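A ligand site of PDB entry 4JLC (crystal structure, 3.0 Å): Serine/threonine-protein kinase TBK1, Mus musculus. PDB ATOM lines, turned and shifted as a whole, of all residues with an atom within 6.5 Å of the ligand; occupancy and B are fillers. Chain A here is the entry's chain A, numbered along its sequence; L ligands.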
ATOM      1  N   LEU A  16     -18.615   2.690 -13.729  1.00  0.00           N
ATOM      2  CA  LEU A  16     -18.168   2.072 -12.488  1.00  0.00           C
ATOM      3  C   LEU A  16     -16.891   2.714 -11.953  1.00  0.00           C
ATOM      4  O   LEU A  16     -16.890   3.873 -11.544  1.00  0.00           O
ATOM      5  CB  LEU A  16     -17.974   0.556 -12.666  1.00  0.00           C
ATOM      6  CG  LEU A  16     -19.221  -0.269 -12.960  1.00  0.00           C
ATOM      7  CD1 LEU A  16     -18.851  -1.725 -13.212  1.00  0.00           C
ATOM      8  CD2 LEU A  16     -20.235  -0.161 -11.833  1.00  0.00           C
ATOM      9  N   GLY A  17     -15.794   1.953 -11.962  1.00  0.00           N
ATOM     10  CA  GLY A  17     -14.534   2.369 -11.370  1.00  0.00           C
ATOM     11  C   GLY A  17     -13.987   3.699 -11.849  1.00  0.00           C
ATOM     12  O   GLY A  17     -13.505   4.497 -11.036  1.00  0.00           O
ATOM     13  N   GLN A  18     -14.053   3.938 -13.159  1.00  0.00           N
ATOM     14  CA  GLN A  18     -13.601   5.184 -13.762  1.00  0.00           C
ATOM     15  C   GLN A  18     -12.110   5.439 -13.528  1.00  0.00           C
ATOM     16  O   GLN A  18     -11.713   5.989 -12.497  1.00  0.00           O
ATOM     17  CB  GLN A  18     -14.435   6.370 -13.266  1.00  0.00           C
ATOM     18  CG  GLN A  18     -14.087   7.696 -13.919  1.00  0.00           C
ATOM     19  CD  GLN A  18     -14.945   8.830 -13.400  1.00  0.00           C
ATOM     20  OE1 GLN A  18     -15.638   8.693 -12.386  1.00  0.00           O
ATOM     21  NE2 GLN A  18     -14.920   9.962 -14.090  1.00  0.00           N
ATOM     22  N   VAL A  24     -14.398   1.861 -16.862  1.00  0.00           N
ATOM     23  CA  VAL A  24     -15.165   0.620 -16.705  1.00  0.00           C
ATOM     24  C   VAL A  24     -16.643   0.901 -16.430  1.00  0.00           C
ATOM     25  O   VAL A  24     -16.994   1.678 -15.542  1.00  0.00           O
ATOM     26  CB  VAL A  24     -14.575  -0.287 -15.601  1.00  0.00           C
ATOM     27  CG1 VAL A  24     -13.415  -1.094 -16.141  1.00  0.00           C
ATOM     28  CG2 VAL A  24     -14.145   0.537 -14.416  1.00  0.00           C
ATOM     29  N   TYR A  36     -22.057  -7.834 -17.410  1.00  0.00           N
ATOM     30  CA  TYR A  36     -20.600  -7.865 -17.486  1.00  0.00           C
ATOM     31  C   TYR A  36     -20.035  -6.462 -17.305  1.00  0.00           C
ATOM     32  O   TYR A  36     -20.670  -5.482 -17.675  1.00  0.00           O
ATOM     33  CB  TYR A  36     -20.122  -8.405 -18.829  1.00  0.00           C
ATOM     34  CG  TYR A  36     -20.538  -9.832 -19.089  1.00  0.00           C
ATOM     35  CD1 TYR A  36     -19.702 -10.890 -18.773  1.00  0.00           C
ATOM     36  CD2 TYR A  36     -21.761 -10.122 -19.669  1.00  0.00           C
ATOM     37  CE1 TYR A  36     -20.071 -12.192 -19.018  1.00  0.00           C
ATOM     38  CE2 TYR A  36     -22.149 -11.422 -19.921  1.00  0.00           C
ATOM     39  CZ  TYR A  36     -21.306 -12.447 -19.591  1.00  0.00           C
ATOM     40  OH  TYR A  36     -21.685 -13.748 -19.839  1.00  0.00           O
ATOM     41  N   ALA A  37     -18.844  -6.376 -16.734  1.00  0.00           N
ATOM     42  CA  ALA A  37     -18.121  -5.118 -16.647  1.00  0.00           C
ATOM     43  C   ALA A  37     -17.323  -4.911 -17.933  1.00  0.00           C
ATOM     44  O   ALA A  37     -16.492  -5.751 -18.283  1.00  0.00           O
ATOM     45  CB  ALA A  37     -17.204  -5.105 -15.444  1.00  0.00           C
ATOM     46  N   LYS A  39     -14.639  -2.594 -20.299  1.00  0.00           N
ATOM     47  CA  LYS A  39     -13.561  -1.625 -20.123  1.00  0.00           C
ATOM     48  C   LYS A  39     -13.204  -0.934 -21.439  1.00  0.00           C
ATOM     49  O   LYS A  39     -12.448  -1.474 -22.245  1.00  0.00           O
ATOM     50  CB  LYS A  39     -12.317  -2.277 -19.516  1.00  0.00           C
ATOM     51  CG  LYS A  39     -11.206  -1.289 -19.178  1.00  0.00           C
ATOM     52  CD  LYS A  39      -9.965  -1.989 -18.653  1.00  0.00           C
ATOM     53  CE  LYS A  39      -8.883  -0.989 -18.295  1.00  0.00           C
ATOM     54  NZ  LYS A  39      -7.604  -1.629 -17.880  1.00  0.00           N
ATOM     55  N   VAL A  69     -10.347 -12.088 -11.662  1.00  0.00           N
ATOM     56  CA  VAL A  69     -11.540 -11.745 -12.447  1.00  0.00           C
ATOM     57  C   VAL A  69     -11.441 -12.333 -13.852  1.00  0.00           C
ATOM     58  O   VAL A  69     -10.404 -12.206 -14.516  1.00  0.00           O
ATOM     59  CB  VAL A  69     -11.783 -10.216 -12.519  1.00  0.00           C
ATOM     60  CG1 VAL A  69     -12.147  -9.653 -11.157  1.00  0.00           C
ATOM     61  CG2 VAL A  69     -10.584  -9.490 -13.107  1.00  0.00           C
ATOM     62  N   LYS A  70     -12.497 -13.005 -14.298  1.00  0.00           N
ATOM     63  CA  LYS A  70     -12.491 -13.635 -15.615  1.00  0.00           C
ATOM     64  C   LYS A  70     -12.541 -12.593 -16.720  1.00  0.00           C
ATOM     65  O   LYS A  70     -13.182 -11.558 -16.589  1.00  0.00           O
ATOM     66  CB  LYS A  70     -13.653 -14.625 -15.774  1.00  0.00           C
ATOM     67  CG  LYS A  70     -13.547 -15.916 -14.953  1.00  0.00           C
ATOM     68  CD  LYS A  70     -14.526 -16.967 -15.464  1.00  0.00           C
ATOM     69  CE  LYS A  70     -14.431 -18.287 -14.704  1.00  0.00           C
ATOM     70  NZ  LYS A  70     -14.653 -18.114 -13.251  1.00  0.00           N
ATOM     71  N   LEU A  71     -11.822 -12.867 -17.816  1.00  0.00           N
ATOM     72  CA  LEU A  71     -11.855 -12.003 -18.993  1.00  0.00           C
ATOM     73  C   LEU A  71     -12.599 -12.733 -20.107  1.00  0.00           C
ATOM     74  O   LEU A  71     -12.061 -13.666 -20.710  1.00  0.00           O
ATOM     75  CB  LEU A  71     -10.436 -11.645 -19.440  1.00  0.00           C
ATOM     76  CG  LEU A  71      -9.510 -11.236 -18.296  1.00  0.00           C
ATOM     77  CD1 LEU A  71      -8.154 -10.819 -18.817  1.00  0.00           C
ATOM     78  CD2 LEU A  71     -10.117 -10.119 -17.466  1.00  0.00           C
ATOM     79  N   MET A  87     -15.279  -8.205 -19.263  1.00  0.00           N
ATOM     80  CA  MET A  87     -14.864  -8.886 -18.034  1.00  0.00           C
ATOM     81  C   MET A  87     -16.028  -9.154 -17.081  1.00  0.00           C
ATOM     82  O   MET A  87     -17.142  -8.664 -17.266  1.00  0.00           O
ATOM     83  CB  MET A  87     -13.794  -8.059 -17.305  1.00  0.00           C
ATOM     84  CG  MET A  87     -13.339  -6.824 -18.077  1.00  0.00           C
ATOM     85  SD  MET A  87     -12.375  -5.690 -17.064  1.00  0.00           S
ATOM     86  CE  MET A  87     -10.885  -6.659 -16.822  1.00  0.00           C
ATOM     87  N   GLU A  88     -15.742  -9.919 -16.028  1.00  0.00           N
ATOM     88  CA  GLU A  88     -16.759 -10.341 -15.068  1.00  0.00           C
ATOM     89  C   GLU A  88     -17.252  -9.214 -14.167  1.00  0.00           C
ATOM     90  O   GLU A  88     -16.455  -8.485 -13.584  1.00  0.00           O
ATOM     91  CB  GLU A  88     -16.192 -11.478 -14.210  1.00  0.00           C
ATOM     92  CG  GLU A  88     -17.000 -11.765 -12.966  1.00  0.00           C
ATOM     93  CD  GLU A  88     -16.280 -12.715 -12.027  1.00  0.00           C
ATOM     94  OE1 GLU A  88     -15.062 -12.906 -12.209  1.00  0.00           O
ATOM     95  OE2 GLU A  88     -16.936 -13.262 -11.121  1.00  0.00           O
ATOM     96  N   PHE A  89     -18.576  -9.076 -14.057  1.00  0.00           N
ATOM     97  CA  PHE A  89     -19.162  -8.046 -13.212  1.00  0.00           C
ATOM     98  C   PHE A  89     -19.192  -8.476 -11.752  1.00  0.00           C
ATOM     99  O   PHE A  89     -19.586  -9.588 -11.428  1.00  0.00           O
ATOM    100  CB  PHE A  89     -20.584  -7.694 -13.699  1.00  0.00           C
ATOM    101  CG  PHE A  89     -21.209  -6.554 -12.952  1.00  0.00           C
ATOM    102  CD1 PHE A  89     -20.743  -5.262 -13.106  1.00  0.00           C
ATOM    103  CD2 PHE A  89     -22.278  -6.771 -12.093  1.00  0.00           C
ATOM    104  CE1 PHE A  89     -21.328  -4.209 -12.420  1.00  0.00           C
ATOM    105  CE2 PHE A  89     -22.863  -5.732 -11.409  1.00  0.00           C
ATOM    106  CZ  PHE A  89     -22.385  -4.448 -11.566  1.00  0.00           C
ATOM    107  N   CYS A  90     -18.774  -7.577 -10.872  1.00  0.00           N
ATOM    108  CA  CYS A  90     -18.739  -7.856  -9.439  1.00  0.00           C
ATOM    109  C   CYS A  90     -19.624  -6.866  -8.691  1.00  0.00           C
ATOM    110  O   CYS A  90     -19.137  -5.823  -8.246  1.00  0.00           O
ATOM    111  CB  CYS A  90     -17.295  -7.785  -8.934  1.00  0.00           C
ATOM    112  SG  CYS A  90     -16.156  -8.868  -9.817  1.00  0.00           S
ATOM    113  N   PRO A  91     -20.907  -7.188  -8.546  1.00  0.00           N
ATOM    114  CA  PRO A  91     -21.944  -6.283  -8.022  1.00  0.00           C
ATOM    115  C   PRO A  91     -21.660  -5.756  -6.611  1.00  0.00           C
ATOM    116  O   PRO A  91     -22.133  -4.669  -6.274  1.00  0.00           O
ATOM    117  CB  PRO A  91     -23.211  -7.151  -8.037  1.00  0.00           C
ATOM    118  CG  PRO A  91     -22.718  -8.561  -8.080  1.00  0.00           C
ATOM    119  CD  PRO A  91     -21.453  -8.519  -8.866  1.00  0.00           C
ATOM    120  N   CYS A  92     -20.898  -6.493  -5.819  1.00  0.00           N
ATOM    121  CA  CYS A  92     -20.649  -6.126  -4.429  1.00  0.00           C
ATOM    122  C   CYS A  92     -19.619  -5.002  -4.296  1.00  0.00           C
ATOM    123  O   CYS A  92     -19.466  -4.429  -3.219  1.00  0.00           O
ATOM    124  CB  CYS A  92     -20.195  -7.340  -3.626  1.00  0.00           C
ATOM    125  SG  CYS A  92     -21.498  -8.569  -3.374  1.00  0.00           S
ATOM    126  N   GLY A  93     -18.919  -4.708  -5.377  1.00  0.00           N
ATOM    127  CA  GLY A  93     -17.878  -3.701  -5.344  1.00  0.00           C
ATOM    128  C   GLY A  93     -16.523  -4.318  -5.032  1.00  0.00           C
ATOM    129  O   GLY A  93     -16.283  -5.479  -5.341  1.00  0.00           O
ATOM    130  N   SER A  94     -15.637  -3.531  -4.415  1.00  0.00           N
ATOM    131  CA  SER A  94     -14.293  -3.999  -4.102  1.00  0.00           C
ATOM    132  C   SER A  94     -14.050  -4.058  -2.586  1.00  0.00           C
ATOM    133  O   SER A  94     -14.960  -3.796  -1.793  1.00  0.00           O
ATOM    134  CB  SER A  94     -13.250  -3.077  -4.751  1.00  0.00           C
ATOM    135  OG  SER A  94     -13.317  -1.783  -4.181  1.00  0.00           O
ATOM    136  N   TYR A  96     -12.229  -2.015  -1.102  1.00  0.00           N
ATOM    137  CA  TYR A  96     -12.354  -0.615  -0.715  1.00  0.00           C
ATOM    138  C   TYR A  96     -13.792  -0.303  -0.344  1.00  0.00           C
ATOM    139  O   TYR A  96     -14.050   0.420   0.623  1.00  0.00           O
ATOM    140  CB  TYR A  96     -11.895   0.295  -1.845  1.00  0.00           C
ATOM    141  CG  TYR A  96     -11.966   1.761  -1.499  1.00  0.00           C
ATOM    142  CD1 TYR A  96     -10.916   2.389  -0.836  1.00  0.00           C
ATOM    143  CD2 TYR A  96     -13.081   2.515  -1.821  1.00  0.00           C
ATOM    144  CE1 TYR A  96     -10.988   3.722  -0.510  1.00  0.00           C
ATOM    145  CE2 TYR A  96     -13.153   3.848  -1.495  1.00  0.00           C
ATOM    146  CZ  TYR A  96     -12.101   4.455  -0.841  1.00  0.00           C
ATOM    147  OH  TYR A  96     -12.170   5.796  -0.521  1.00  0.00           O
ATOM    148  N   THR A  97     -14.738  -0.844  -1.117  1.00  0.00           N
ATOM    149  CA  THR A  97     -16.155  -0.670  -0.850  1.00  0.00           C
ATOM    150  C   THR A  97     -16.523  -1.258   0.510  1.00  0.00           C
ATOM    151  O   THR A  97     -17.261  -0.644   1.284  1.00  0.00           O
ATOM    152  CB  THR A  97     -17.017  -1.344  -1.931  1.00  0.00           C
ATOM    153  OG1 THR A  97     -16.483  -1.067  -3.220  1.00  0.00           O
ATOM    154  CG2 THR A  97     -18.449  -0.843  -1.862  1.00  0.00           C
ATOM    155  N   GLY A 140      -8.732  -1.037  -3.726  1.00  0.00           N
ATOM    156  CA  GLY A 140      -9.395  -0.511  -4.904  1.00  0.00           C
ATOM    157  C   GLY A 140      -9.539  -1.504  -6.047  1.00  0.00           C
ATOM    158  O   GLY A 140     -10.569  -1.532  -6.738  1.00  0.00           O
ATOM    159  N   MET A 143     -11.753  -6.955  -6.193  1.00  0.00           N
ATOM    160  CA  MET A 143     -13.209  -7.019  -6.295  1.00  0.00           C
ATOM    161  C   MET A 143     -13.802  -8.094  -5.397  1.00  0.00           C
ATOM    162  O   MET A 143     -13.146  -9.072  -5.048  1.00  0.00           O
ATOM    163  CB  MET A 143     -13.631  -7.261  -7.745  1.00  0.00           C
ATOM    164  CG  MET A 143     -13.002  -6.286  -8.722  1.00  0.00           C
ATOM    165  SD  MET A 143     -13.257  -4.575  -8.229  1.00  0.00           S
ATOM    166  CE  MET A 143     -15.051  -4.514  -8.144  1.00  0.00           C
ATOM    167  N   THR A 157      -7.785  -7.823  -9.917  1.00  0.00           N
ATOM    168  CA  THR A 157      -7.970  -7.286 -11.257  1.00  0.00           C
ATOM    169  C   THR A 157      -6.841  -6.311 -11.550  1.00  0.00           C
ATOM    170  O   THR A 157      -5.974  -6.097 -10.695  1.00  0.00           O
ATOM    171  CB  THR A 157      -9.325  -6.581 -11.398  1.00  0.00           C
ATOM    172  OG1 THR A 157      -9.562  -6.280 -12.782  1.00  0.00           O
ATOM    173  CG2 THR A 157      -9.358  -5.292 -10.592  1.00  0.00           C
ATOM    174  N   ASP A 158      -6.832  -5.758 -12.754  1.00  0.00           N
ATOM    175  CA  ASP A 158      -5.872  -4.728 -13.128  1.00  0.00           C
ATOM    176  C   ASP A 158      -4.435  -5.222 -12.994  1.00  0.00           C
ATOM    177  O   ASP A 158      -3.771  -4.997 -11.984  1.00  0.00           O
ATOM    178  CB  ASP A 158      -6.106  -3.466 -12.285  1.00  0.00           C
ATOM    179  CG  ASP A 158      -5.140  -2.353 -12.633  1.00  0.00           C
ATOM    180  OD1 ASP A 158      -4.146  -2.174 -11.882  1.00  0.00           O
ATOM    181  OD2 ASP A 158      -5.373  -1.651 -13.639  1.00  0.00           O
HETATM  182  C1  LIG L   1     -18.731   0.987  -5.264  1.00  0.00           C
HETATM  183  N1  LIG L   1     -18.152  -2.952  -9.827  1.00  0.00           N
HETATM  184  O1  LIG L   1     -19.916   1.372  -5.450  1.00  0.00           O
HETATM  185  C2  LIG L   1     -18.098   0.040  -6.236  1.00  0.00           C
HETATM  186  N2  LIG L   1     -15.937  -5.978 -12.328  1.00  0.00           N
HETATM  187  O2  LIG L   1     -18.081   1.405  -4.265  1.00  0.00           O
HETATM  188  C3  LIG L   1     -18.801  -0.145  -7.543  1.00  0.00           C
HETATM  189  O3  LIG L   1     -17.868  -5.137 -11.243  1.00  0.00           O
HETATM  190  C4  LIG L   1     -18.301  -1.141  -8.543  1.00  0.00           C
HETATM  191  C5  LIG L   1     -18.901  -2.347  -8.897  1.00  0.00           C
HETATM  192  C6  LIG L   1     -20.184  -2.863  -8.332  1.00  0.00           C
HETATM  193  C7  LIG L   1     -17.140  -1.071  -9.308  1.00  0.00           C
HETATM  194  C8  LIG L   1     -16.146   0.039  -9.299  1.00  0.00           C
HETATM  195  C9  LIG L   1     -17.072  -2.214 -10.094  1.00  0.00           C
HETATM  196  C10 LIG L   1     -15.969  -2.489 -11.069  1.00  0.00           C
HETATM  197  C11 LIG L   1     -15.757  -3.865 -11.640  1.00  0.00           C
HETATM  198  C12 LIG L   1     -16.594  -4.994 -11.716  1.00  0.00           C
HETATM  199  C13 LIG L   1     -14.557  -4.256 -12.286  1.00  0.00           C
HETATM  200  C14 LIG L   1     -14.700  -5.568 -12.691  1.00  0.00           C
HETATM  201  C15 LIG L   1     -13.649  -6.209 -13.361  1.00  0.00           C
HETATM  202  C16 LIG L   1     -12.464  -5.546 -13.607  1.00  0.00           C
HETATM  203  C17 LIG L   1     -12.315  -4.228 -13.191  1.00  0.00           C
HETATM  204  C18 LIG L   1     -13.348  -3.579 -12.536  1.00  0.00           C
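The backbone NH (N) of Cys 90 is in hydrogen-bond range of an oxygen (O3) of the ligand (2.6 Å).
A nitrogen (N1) of the ligand sits close to the backbone carbonyl oxygen of Cys 90, at 3.4 Å.
The backbone carbonyl oxygen of Glu 88 is in hydrogen-bond range of a nitrogen (N2) of the ligand, at 2.9 Å.
An oxygen (O2) of the ligand is in hydrogen-bond range of the side-chain hydroxyl of Thr 97.
The side-chain sulfur (SG) of Cys 90 is in hydrogen-bond range of the backbone carbonyl oxygen (O) of Glu 88, at 3.8 Å.
N of Glu 88 sits at hydrogen-bond distance from O of Lys 70, 3.1 Å away.
N of Ser 94 sits at hydrogen-bond distance from OG1 of Thr 97, at 2.9 Å.
The backbone carbonyl oxygen (O) of Met 87 sits at hydrogen-bond distance from the backbone NH (N) of Ala 37 (2.9 Å).
The backbone NH (N) of Leu 16 sits at hydrogen-bond distance from the backbone carbonyl oxygen (O) of Val 24 (2.6 Å).
CD1 of Leu 16 touches C9 of the ligand (3.6 Å).
Gly 17 touches the ligand.
Ala 37 touches the ligand.
Met 87 touches the ligand.
Phe 89 touches the ligand.
Pro 91 touches the ligand (O to C6, 3.4 Å).
N of Gly 93 touches C6 of the ligand (3.7 Å).
Met 143 touches the ligand (CE to C11, 3.6 Å).
Thr 157 touches the ligand (OG1 to C16, 3.1 Å).
Hydrophobic or aromatic side chains within 4 Å of the ligand: Leu 16, Ala 37, Met 87, Phe 89 and Met 143.
The nearest printed residue that does not touch the ligand is Val 69 (4.4 Å).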
